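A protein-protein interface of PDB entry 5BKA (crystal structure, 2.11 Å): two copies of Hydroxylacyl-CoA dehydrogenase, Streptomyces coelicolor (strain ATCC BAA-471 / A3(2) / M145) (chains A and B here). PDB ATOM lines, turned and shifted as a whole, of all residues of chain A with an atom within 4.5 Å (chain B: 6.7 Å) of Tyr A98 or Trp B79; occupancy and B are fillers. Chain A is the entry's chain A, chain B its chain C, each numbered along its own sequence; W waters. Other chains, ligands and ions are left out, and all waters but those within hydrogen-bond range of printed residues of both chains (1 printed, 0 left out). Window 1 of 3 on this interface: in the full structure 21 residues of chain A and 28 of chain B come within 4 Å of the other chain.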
ATOM      1  N   TRP A  79      25.981  15.691  22.657  1.00  0.00           N
ATOM      2  CA  TRP A  79      24.814  15.809  21.795  1.00  0.00           C
ATOM      3  C   TRP A  79      23.552  15.393  22.541  1.00  0.00           C
ATOM      4  O   TRP A  79      23.563  14.430  23.308  1.00  0.00           O
ATOM      5  CB  TRP A  79      24.991  14.939  20.548  1.00  0.00           C
ATOM      6  CG  TRP A  79      25.856  15.567  19.505  1.00  0.00           C
ATOM      7  CD1 TRP A  79      27.086  16.130  19.689  1.00  0.00           C
ATOM      8  CD2 TRP A  79      25.553  15.706  18.113  1.00  0.00           C
ATOM      9  NE1 TRP A  79      27.570  16.609  18.496  1.00  0.00           N
ATOM     10  CE2 TRP A  79      26.647  16.362  17.512  1.00  0.00           C
ATOM     11  CE3 TRP A  79      24.466  15.337  17.315  1.00  0.00           C
ATOM     12  CZ2 TRP A  79      26.683  16.660  16.151  1.00  0.00           C
ATOM     13  CZ3 TRP A  79      24.502  15.636  15.962  1.00  0.00           C
ATOM     14  CH2 TRP A  79      25.604  16.289  15.394  1.00  0.00           C
ATOM     15  N   PHE A  80      22.468  16.132  22.319  1.00  0.00           N
ATOM     16  CA  PHE A  80      21.155  15.809  22.864  1.00  0.00           C
ATOM     17  C   PHE A  80      20.204  15.442  21.732  1.00  0.00           C
ATOM     18  O   PHE A  80      20.401  15.834  20.581  1.00  0.00           O
ATOM     19  CB  PHE A  80      20.567  16.986  23.655  1.00  0.00           C
ATOM     20  CG  PHE A  80      21.051  17.085  25.078  1.00  0.00           C
ATOM     21  CD1 PHE A  80      22.249  16.512  25.469  1.00  0.00           C
ATOM     22  CD2 PHE A  80      20.304  17.772  26.023  1.00  0.00           C
ATOM     23  CE1 PHE A  80      22.690  16.617  26.778  1.00  0.00           C
ATOM     24  CE2 PHE A  80      20.738  17.880  27.332  1.00  0.00           C
ATOM     25  CZ  PHE A  80      21.932  17.302  27.710  1.00  0.00           C
ATOM     26  N   ASP A  81      19.154  14.694  22.071  1.00  0.00           N
ATOM     27  CA  ASP A  81      18.143  14.334  21.084  1.00  0.00           C
ATOM     28  C   ASP A  81      16.873  13.880  21.788  1.00  0.00           C
ATOM     29  O   ASP A  81      16.917  13.378  22.915  1.00  0.00           O
ATOM     30  CB  ASP A  81      18.634  13.237  20.136  1.00  0.00           C
ATOM     31  CG  ASP A  81      17.826  13.170  18.852  1.00  0.00           C
ATOM     32  OD1 ASP A  81      17.785  14.180  18.122  1.00  0.00           O
ATOM     33  OD2 ASP A  81      17.233  12.108  18.571  1.00  0.00           O
ATOM     34  N   HIS A  82      15.744  14.071  21.103  1.00  0.00           N
ATOM     35  CA  HIS A  82      14.443  13.539  21.522  1.00  0.00           C
ATOM     36  C   HIS A  82      14.059  14.000  22.928  1.00  0.00           C
ATOM     37  O   HIS A  82      13.699  13.198  23.794  1.00  0.00           O
ATOM     38  CB  HIS A  82      14.425  12.013  21.425  1.00  0.00           C
ATOM     39  CG  HIS A  82      14.288  11.501  20.026  1.00  0.00           C
ATOM     40  ND1 HIS A  82      13.539  12.148  19.068  1.00  0.00           N
ATOM     41  CD2 HIS A  82      14.806  10.404  19.422  1.00  0.00           C
ATOM     42  CE1 HIS A  82      13.600  11.472  17.934  1.00  0.00           C
ATOM     43  NE2 HIS A  82      14.363  10.410  18.121  1.00  0.00           N
ATOM     44  N   SER A  97      15.887  13.468  27.948  1.00  0.00           N
ATOM     45  CA  SER A  97      16.541  13.593  26.655  1.00  0.00           C
ATOM     46  C   SER A  97      17.566  12.485  26.473  1.00  0.00           C
ATOM     47  O   SER A  97      18.147  11.991  27.441  1.00  0.00           O
ATOM     48  CB  SER A  97      17.249  14.950  26.520  1.00  0.00           C
ATOM     49  OG  SER A  97      16.328  16.024  26.489  1.00  0.00           O
ATOM     50  N   TYR A  98      17.780  12.100  25.217  1.00  0.00           N
ATOM     51  CA  TYR A  98      18.927  11.282  24.863  1.00  0.00           C
ATOM     52  C   TYR A  98      20.180  12.145  24.854  1.00  0.00           C
ATOM     53  O   TYR A  98      20.145  13.319  24.478  1.00  0.00           O
ATOM     54  CB  TYR A  98      18.748  10.644  23.482  1.00  0.00           C
ATOM     55  CG  TYR A  98      17.654   9.606  23.369  1.00  0.00           C
ATOM     56  CD1 TYR A  98      16.955   9.166  24.483  1.00  0.00           C
ATOM     57  CD2 TYR A  98      17.328   9.061  22.133  1.00  0.00           C
ATOM     58  CE1 TYR A  98      15.956   8.215  24.369  1.00  0.00           C
ATOM     59  CE2 TYR A  98      16.335   8.112  22.009  1.00  0.00           C
ATOM     60  CZ  TYR A  98      15.652   7.691  23.127  1.00  0.00           C
ATOM     61  OH  TYR A  98      14.663   6.745  23.002  1.00  0.00           O
ATOM     62  N   CYS A  99      21.305  11.548  25.232  1.00  0.00           N
ATOM     63  CA  CYS A  99      22.583  12.233  25.122  1.00  0.00           C
ATOM     64  C   CYS A  99      23.654  11.254  24.671  1.00  0.00           C
ATOM     65  O   CYS A  99      23.704  10.112  25.137  1.00  0.00           O
ATOM     66  CB  CYS A  99      22.993  12.888  26.453  1.00  0.00           C
ATOM     67  SG  CYS A  99      24.652  13.626  26.451  1.00  0.00           S
ATOM     68  N   LEU A 100      24.523  11.716  23.776  1.00  0.00           N
ATOM     69  CA  LEU A 100      25.634  10.925  23.257  1.00  0.00           C
ATOM     70  C   LEU A 100      26.893  11.772  23.348  1.00  0.00           C
ATOM     71  O   LEU A 100      26.942  12.879  22.800  1.00  0.00           O
ATOM     72  CB  LEU A 100      25.387  10.475  21.813  1.00  0.00           C
ATOM     73  CG  LEU A 100      26.535   9.718  21.125  1.00  0.00           C
ATOM     74  CD1 LEU A 100      26.825   8.385  21.811  1.00  0.00           C
ATOM     75  CD2 LEU A 100      26.245   9.510  19.643  1.00  0.00           C
ATOM     76  N   CYS A 117      23.503   8.197  26.982  1.00  0.00           N
ATOM     77  CA  CYS A 117      22.902   8.469  28.282  1.00  0.00           C
ATOM     78  C   CYS A 117      21.467   8.953  28.146  1.00  0.00           C
ATOM     79  O   CYS A 117      21.041   9.430  27.091  1.00  0.00           O
ATOM     80  CB  CYS A 117      23.695   9.519  29.087  1.00  0.00           C
ATOM     81  SG  CYS A 117      25.488   9.445  28.916  1.00  0.00           S
ATOM     82  N   LEU A 118      20.730   8.824  29.245  1.00  0.00           N
ATOM     83  CA  LEU A 118      19.445   9.482  29.433  1.00  0.00           C
ATOM     84  C   LEU A 118      19.643  10.653  30.385  1.00  0.00           C
ATOM     85  O   LEU A 118      20.288  10.508  31.428  1.00  0.00           O
ATOM     86  CB  LEU A 118      18.402   8.514  29.995  1.00  0.00           C
ATOM     87  CG  LEU A 118      17.801   7.467  29.054  1.00  0.00           C
ATOM     88  CD1 LEU A 118      16.753   6.638  29.783  1.00  0.00           C
ATOM     89  CD2 LEU A 118      17.202   8.121  27.823  1.00  0.00           C
ATOM     90  N   GLY B  19       9.874  12.926  19.929  1.00  0.00           N
ATOM     91  CA  GLY B  19      10.583  12.639  21.166  1.00  0.00           C
ATOM     92  C   GLY B  19       9.867  11.611  22.023  1.00  0.00           C
ATOM     93  O   GLY B  19      10.472  10.643  22.491  1.00  0.00           O
ATOM     94  N   MET B  22       9.608   8.039  19.929  1.00  0.00           N
ATOM     95  CA  MET B  22      10.831   7.244  19.846  1.00  0.00           C
ATOM     96  C   MET B  22      11.251   6.678  21.195  1.00  0.00           C
ATOM     97  O   MET B  22      11.770   5.564  21.274  1.00  0.00           O
ATOM     98  CB  MET B  22      11.971   8.075  19.258  1.00  0.00           C
ATOM     99  CG  MET B  22      11.960   8.102  17.752  1.00  0.00           C
ATOM    100  SD  MET B  22      11.413   6.363  17.087  1.00  0.00           S
ATOM    101  CE  MET B  22      10.027   6.939  15.890  1.00  0.00           C
ATOM    102  N   GLN B  23      11.037   7.455  22.260  1.00  0.00           N
ATOM    103  CA  GLN B  23      11.343   6.960  23.597  1.00  0.00           C
ATOM    104  C   GLN B  23      10.465   5.768  23.958  1.00  0.00           C
ATOM    105  O   GLN B  23      10.904   4.872  24.686  1.00  0.00           O
ATOM    106  CB  GLN B  23      11.188   8.086  24.621  1.00  0.00           C
ATOM    107  CG  GLN B  23      12.348   9.078  24.612  1.00  0.00           C
ATOM    108  CD  GLN B  23      12.343  10.015  25.808  1.00  0.00           C
ATOM    109  OE1 GLN B  23      11.871   9.663  26.888  1.00  0.00           O
ATOM    110  NE2 GLN B  23      12.877  11.217  25.619  1.00  0.00           N
ATOM    111  N   LYS B  24       9.224   5.746  23.466  1.00  0.00           N
ATOM    112  CA  LYS B  24       8.380   4.564  23.610  1.00  0.00           C
ATOM    113  C   LYS B  24       8.975   3.369  22.871  1.00  0.00           C
ATOM    114  O   LYS B  24       9.117   2.282  23.444  1.00  0.00           O
ATOM    115  CB  LYS B  24       6.970   4.865  23.104  1.00  0.00           C
ATOM    116  N   LEU B  25       9.302   3.549  21.587  1.00  0.00           N
ATOM    117  CA  LEU B  25       9.898   2.472  20.800  1.00  0.00           C
ATOM    118  C   LEU B  25      11.164   1.938  21.459  1.00  0.00           C
ATOM    119  O   LEU B  25      11.326   0.724  21.631  1.00  0.00           O
ATOM    120  CB  LEU B  25      10.196   2.961  19.381  1.00  0.00           C
ATOM    121  CG  LEU B  25      10.924   1.965  18.471  1.00  0.00           C
ATOM    122  CD1 LEU B  25      10.030   0.780  18.133  1.00  0.00           C
ATOM    123  CD2 LEU B  25      11.415   2.648  17.204  1.00  0.00           C
ATOM    124  N   ASP B  26      12.078   2.835  21.835  1.00  0.00           N
ATOM    125  CA  ASP B  26      13.336   2.408  22.436  1.00  0.00           C
ATOM    126  C   ASP B  26      13.146   1.826  23.830  1.00  0.00           C
ATOM    127  O   ASP B  26      14.016   1.080  24.297  1.00  0.00           O
ATOM    128  CB  ASP B  26      14.317   3.578  22.475  1.00  0.00           C
ATOM    129  CG  ASP B  26      14.751   4.012  21.090  1.00  0.00           C
ATOM    130  OD1 ASP B  26      14.734   3.165  20.172  1.00  0.00           O
ATOM    131  OD2 ASP B  26      15.105   5.197  20.915  1.00  0.00           O
ATOM    132  N   GLY B  27      12.040   2.144  24.499  1.00  0.00           N
ATOM    133  CA  GLY B  27      11.696   1.520  25.757  1.00  0.00           C
ATOM    134  C   GLY B  27      10.904   0.239  25.614  1.00  0.00           C
ATOM    135  O   GLY B  27      10.329  -0.238  26.598  1.00  0.00           O
ATOM    136  N   GLN B  75      20.303  -2.258  24.473  1.00  0.00           N
ATOM    137  CA  GLN B  75      19.472  -1.062  24.558  1.00  0.00           C
ATOM    138  C   GLN B  75      19.625  -0.270  23.269  1.00  0.00           C
ATOM    139  O   GLN B  75      20.731   0.165  22.933  1.00  0.00           O
ATOM    140  CB  GLN B  75      19.854  -0.200  25.765  1.00  0.00           C
ATOM    141  CG  GLN B  75      19.164   1.156  25.793  1.00  0.00           C
ATOM    142  CD  GLN B  75      17.666   1.043  26.020  1.00  0.00           C
ATOM    143  OE1 GLN B  75      17.218   0.538  27.048  1.00  0.00           O
ATOM    144  NE2 GLN B  75      16.885   1.514  25.055  1.00  0.00           N
ATOM    145  N   ARG B  76      18.522  -0.084  22.550  1.00  0.00           N
ATOM    146  CA  ARG B  76      18.526   0.627  21.281  1.00  0.00           C
ATOM    147  C   ARG B  76      18.103   2.079  21.469  1.00  0.00           C
ATOM    148  O   ARG B  76      17.341   2.409  22.380  1.00  0.00           O
ATOM    149  CB  ARG B  76      17.590  -0.050  20.279  1.00  0.00           C
ATOM    150  CG  ARG B  76      18.035  -1.433  19.851  1.00  0.00           C
ATOM    151  CD  ARG B  76      17.582  -1.731  18.437  1.00  0.00           C
ATOM    152  NE  ARG B  76      18.710  -2.007  17.555  1.00  0.00           N
ATOM    153  CZ  ARG B  76      18.657  -1.936  16.229  1.00  0.00           C
ATOM    154  NH1 ARG B  76      17.527  -1.593  15.623  1.00  0.00           N
ATOM    155  NH2 ARG B  76      19.736  -2.207  15.509  1.00  0.00           N
ATOM    156  N   ARG B  77      18.624   2.946  20.600  1.00  0.00           N
ATOM    157  CA  ARG B  77      18.246   4.355  20.561  1.00  0.00           C
ATOM    158  C   ARG B  77      18.117   4.788  19.109  1.00  0.00           C
ATOM    159  O   ARG B  77      19.055   4.615  18.325  1.00  0.00           O
ATOM    160  CB  ARG B  77      19.274   5.238  21.281  1.00  0.00           C
ATOM    161  CG  ARG B  77      19.443   4.939  22.765  1.00  0.00           C
ATOM    162  CD  ARG B  77      18.219   5.344  23.571  1.00  0.00           C
ATOM    163  NE  ARG B  77      18.361   4.984  24.980  1.00  0.00           N
ATOM    164  CZ  ARG B  77      17.343   4.757  25.805  1.00  0.00           C
ATOM    165  NH1 ARG B  77      16.095   4.852  25.367  1.00  0.00           N
ATOM    166  NH2 ARG B  77      17.574   4.434  27.070  1.00  0.00           N
ATOM    167  N   HIS B  78      16.969   5.367  18.759  1.00  0.00           N
ATOM    168  CA  HIS B  78      16.696   5.838  17.401  1.00  0.00           C
ATOM    169  C   HIS B  78      16.777   7.362  17.394  1.00  0.00           C
ATOM    170  O   HIS B  78      15.800   8.045  17.714  1.00  0.00           O
ATOM    171  CB  HIS B  78      15.330   5.358  16.922  1.00  0.00           C
ATOM    172  CG  HIS B  78      15.273   3.893  16.616  1.00  0.00           C
ATOM    173  ND1 HIS B  78      15.317   2.925  17.597  1.00  0.00           N
ATOM    174  CD2 HIS B  78      15.172   3.230  15.439  1.00  0.00           C
ATOM    175  CE1 HIS B  78      15.246   1.731  17.037  1.00  0.00           C
ATOM    176  NE2 HIS B  78      15.158   1.888  15.728  1.00  0.00           N
ATOM    177  N   TRP B  79      17.938   7.890  17.014  1.00  0.00           N
ATOM    178  CA  TRP B  79      18.135   9.331  16.949  1.00  0.00           C
ATOM    179  C   TRP B  79      17.550   9.897  15.662  1.00  0.00           C
ATOM    180  O   TRP B  79      17.669   9.295  14.593  1.00  0.00           O
ATOM    181  CB  TRP B  79      19.626   9.665  17.035  1.00  0.00           C
ATOM    182  CG  TRP B  79      20.158   9.653  18.435  1.00  0.00           C
ATOM    183  CD1 TRP B  79      20.030   8.651  19.350  1.00  0.00           C
ATOM    184  CD2 TRP B  79      20.899  10.695  19.080  1.00  0.00           C
ATOM    185  NE1 TRP B  79      20.646   9.003  20.526  1.00  0.00           N
ATOM    186  CE2 TRP B  79      21.187  10.254  20.386  1.00  0.00           C
ATOM    187  CE3 TRP B  79      21.352  11.955  18.677  1.00  0.00           C
ATOM    188  CZ2 TRP B  79      21.901  11.030  21.296  1.00  0.00           C
ATOM    189  CZ3 TRP B  79      22.059  12.727  19.584  1.00  0.00           C
ATOM    190  CH2 TRP B  79      22.328  12.260  20.877  1.00  0.00           C
ATOM    191  N   PHE B  80      16.915  11.061  15.770  1.00  0.00           N
ATOM    192  CA  PHE B  80      16.386  11.793  14.629  1.00  0.00           C
ATOM    193  C   PHE B  80      17.163  13.090  14.449  1.00  0.00           C
ATOM    194  O   PHE B  80      17.778  13.603  15.386  1.00  0.00           O
ATOM    195  CB  PHE B  80      14.896  12.112  14.809  1.00  0.00           C
ATOM    196  CG  PHE B  80      13.968  11.021  14.348  1.00  0.00           C
ATOM    197  CD1 PHE B  80      14.381   9.700  14.315  1.00  0.00           C
ATOM    198  CD2 PHE B  80      12.674  11.322  13.958  1.00  0.00           C
ATOM    199  CE1 PHE B  80      13.518   8.700  13.897  1.00  0.00           C
ATOM    200  CE2 PHE B  80      11.807  10.328  13.539  1.00  0.00           C
ATOM    201  CZ  PHE B  80      12.230   9.016  13.509  1.00  0.00           C
ATOM    202  N   ASP B  81      17.121  13.627  13.231  1.00  0.00           N
ATOM    203  CA  ASP B  81      17.789  14.890  12.951  1.00  0.00           C
ATOM    204  C   ASP B  81      17.217  15.500  11.684  1.00  0.00           C
ATOM    205  O   ASP B  81      16.769  14.787  10.782  1.00  0.00           O
ATOM    206  CB  ASP B  81      19.302  14.705  12.796  1.00  0.00           C
ATOM    207  CG  ASP B  81      20.088  15.929  13.224  1.00  0.00           C
ATOM    208  OD1 ASP B  81      20.107  16.228  14.434  1.00  0.00           O
ATOM    209  OD2 ASP B  81      20.691  16.587  12.349  1.00  0.00           O
ATOM    210  N   TYR B  98      16.280  12.626   9.192  1.00  0.00           N
ATOM    211  CA  TYR B  98      17.376  11.674   9.305  1.00  0.00           C
ATOM    212  C   TYR B  98      17.163  10.787  10.524  1.00  0.00           C
ATOM    213  O   TYR B  98      16.602  11.215  11.536  1.00  0.00           O
ATOM    214  CB  TYR B  98      18.719  12.395   9.438  1.00  0.00           C
ATOM    215  CG  TYR B  98      19.155  13.192   8.232  1.00  0.00           C
ATOM    216  CD1 TYR B  98      18.460  13.125   7.030  1.00  0.00           C
ATOM    217  CD2 TYR B  98      20.275  14.012   8.295  1.00  0.00           C
ATOM    218  CE1 TYR B  98      18.865  13.854   5.930  1.00  0.00           C
ATOM    219  CE2 TYR B  98      20.689  14.743   7.201  1.00  0.00           C
ATOM    220  CZ  TYR B  98      19.980  14.662   6.021  1.00  0.00           C
ATOM    221  OH  TYR B  98      20.393  15.391   4.933  1.00  0.00           O
ATOM    222  N   CYS B  99      17.622   9.543  10.431  1.00  0.00           N
ATOM    223  CA  CYS B  99      17.610   8.668  11.592  1.00  0.00           C
ATOM    224  C   CYS B  99      18.897   7.865  11.651  1.00  0.00           C
ATOM    225  O   CYS B  99      19.405   7.407  10.624  1.00  0.00           O
ATOM    226  CB  CYS B  99      16.406   7.714  11.580  1.00  0.00           C
ATOM    227  SG  CYS B  99      16.353   6.565  12.997  1.00  0.00           S
ATOM    228  N   LEU B 100      19.423   7.714  12.866  1.00  0.00           N
ATOM    229  CA  LEU B 100      20.628   6.939  13.124  1.00  0.00           C
ATOM    230  C   LEU B 100      20.339   6.015  14.294  1.00  0.00           C
ATOM    231  O   LEU B 100      19.967   6.482  15.376  1.00  0.00           O
ATOM    232  CB  LEU B 100      21.828   7.841  13.429  1.00  0.00           C
ATOM    233  CG  LEU B 100      23.135   7.120  13.758  1.00  0.00           C
ATOM    234  CD1 LEU B 100      23.607   6.294  12.566  1.00  0.00           C
ATOM    235  CD2 LEU B 100      24.212   8.105  14.196  1.00  0.00           C
ATOM    236  N   VAL B 101      20.496   4.716  14.078  1.00  0.00           N
ATOM    237  CA  VAL B 101      20.200   3.720  15.100  1.00  0.00           C
ATOM    238  C   VAL B 101      21.458   3.454  15.914  1.00  0.00           C
ATOM    239  O   VAL B 101      22.537   3.225  15.356  1.00  0.00           O
ATOM    240  CB  VAL B 101      19.667   2.425  14.468  1.00  0.00           C
ATOM    241  CG1 VAL B 101      19.352   1.404  15.551  1.00  0.00           C
ATOM    242  CG2 VAL B 101      18.432   2.714  13.626  1.00  0.00           C
ATOM    243  N   LEU B 102      21.317   3.495  17.234  1.00  0.00           N
ATOM    244  CA  LEU B 102      22.376   3.146  18.168  1.00  0.00           C
ATOM    245  C   LEU B 102      22.024   1.821  18.828  1.00  0.00           C
ATOM    246  O   LEU B 102      20.874   1.613  19.229  1.00  0.00           O
ATOM    247  CB  LEU B 102      22.554   4.229  19.236  1.00  0.00           C
ATOM    248  CG  LEU B 102      23.441   5.441  18.941  1.00  0.00           C
ATOM    249  CD1 LEU B 102      22.869   6.292  17.814  1.00  0.00           C
ATOM    250  CD2 LEU B 102      23.624   6.280  20.202  1.00  0.00           C
ATOM    251  N   VAL B 119      13.499   8.840   7.215  1.00  0.00           N
ATOM    252  CA  VAL B 119      12.170   8.530   7.727  1.00  0.00           C
ATOM    253  C   VAL B 119      11.174   9.413   6.989  1.00  0.00           C
ATOM    254  O   VAL B 119      11.132  10.630   7.203  1.00  0.00           O
ATOM    255  CB  VAL B 119      12.078   8.737   9.245  1.00  0.00           C
ATOM    256  CG1 VAL B 119      10.676   8.420   9.734  1.00  0.00           C
ATOM    257  CG2 VAL B 119      13.104   7.873   9.961  1.00  0.00           C
HETATM  258  O   HOH W   1      14.772  14.823  16.679  1.00  0.00           O
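Among the printed residues, merely in contact across the chains: Trp A79 with Trp B79 (3.5 Å), Phe A80 with Trp B79 (3.7 Å), Asp A81 with Trp B79 (3.3 Å), His A82 with Gly B19 (3.7 Å), His A82 with Met B22 (3.4 Å), His A82 with Phe B80 (3.4 Å), Tyr A98 with Met B22 (3.6 Å), Tyr A98 with Gln B23 (3.4 Å), Tyr A98 with Trp B79 (3.7 Å), Cys A99 with Trp B79 (3.8 Å), Leu A100 with Trp B79 (3.6 Å) and Leu A118 with Arg B77 (3.6 Å).
Trp B79 touches its own counterpart, Trp A79.
Phe A80 touches Trp B79, but with the chains exchanged Trp A79 does not touch Phe B80 (7.0 Å).
Asp A81 touches Phe B80, but with the chains exchanged Phe A80 does not touch Asp B81 (6.2 Å).
Cys A99 touches Trp B79, but with the chains exchanged Trp A79 does not touch Cys B99 (10.5 Å).
6 positions are printed for both chains.
Of the 17 pairs that touch across the chains among the printed residues, 1 has its exchanged pair printed and touching as well.
Printed residues of chain B that touch a printed residue of chain A: Gly B19, Met B22, Gln B23, Asp B26, Arg B77, His B78, Trp B79 and Phe B80.
Printed residues of chain A that touch a printed residue of chain B: Trp A79, Phe A80, Asp A81, His A82, Tyr A98, Cys A99, Leu A100 and Leu A118.
Among the printed residues, no Asp or Glu carboxylate lies within 4 Å of a Lys or Arg side-chain nitrogen of the other chain.
O of His A82 sits at hydrogen-bond distance from NE2 of Gln B23, 2.8 Å away.
The side-chain carboxylate (OD2) of Asp B26 sits at hydrogen-bond distance from the side-chain hydroxyl (OH) of Tyr A98, 2.6 Å away.
A ring nitrogen (NE2) of His A82 sits at hydrogen-bond distance from the backbone carbonyl oxygen (O) of His B78, 2.8 Å away.
NH1 of Arg B77 lies within hydrogen-bond range of OH of Tyr A98.
The side-chain carboxylate (OD2) of Asp A81 is in hydrogen-bond range of the backbone NH (N) of Phe B80 (3.0 Å).
Of the printed residues of chain B, Asp A81 touches Trp B79 and Phe B80.
Tyr A98 touches just these residues of chain B: Met B22 (3.6 Å), Gln B23 (3.4 Å), Asp B26 (2.6 Å), Arg B77 (3.4 Å) and Trp B79 (3.7 Å).
Of the printed residues of chain A, Gly B19 touches His A82 (3.7 Å).
Of the printed residues of chain A, Gln B23 touches His A82 and Tyr A98.
Arg B76 touches none of the printed residues of chain A.
Trp B79 touches just these residues of chain A: Trp A79 (3.5 Å), Phe A80 (3.7 Å), Asp A81 (3.3 Å), Tyr A98 (3.7 Å), Cys A99 (3.8 Å) and Leu A100 (3.6 Å).
Val B119 touches none of the printed residues of chain A.
The nearest residue of chain A that does not touch Trp B79 is His A82 (4.1 Å).
The nearest printed residue of chain B that does not touch Phe A80 is Asp B81 (6.2 Å).
Water W1 lies within hydrogen-bond range of the side-chain carboxylate of Asp A81 (3.4 Å) and the backbone carbonyl oxygen of Phe B80 (3.5 Å).
A ring nitrogen (NE2) of His A82 lies close to the side-chain carboxylate (OD2) of Asp A81.
The backbone carbonyl oxygen of Trp B79 lies within hydrogen-bond range of the backbone NH of Leu B100, at 2.9 Å.
NE2 of Gln B75 is in hydrogen-bond range of O of Asp B26.
The backbone carbonyl oxygen (O) of Trp A79 lies close to the side-chain sulfur (SG) of Cys A99, at 3.4 Å.
O of Cys A99 is in hydrogen-bond range of N of Cys A117 (2.7 Å).
The side-chain amide nitrogen of Gln B75 lies close to the guanidinium group of Arg B77, at 3.4 Å.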
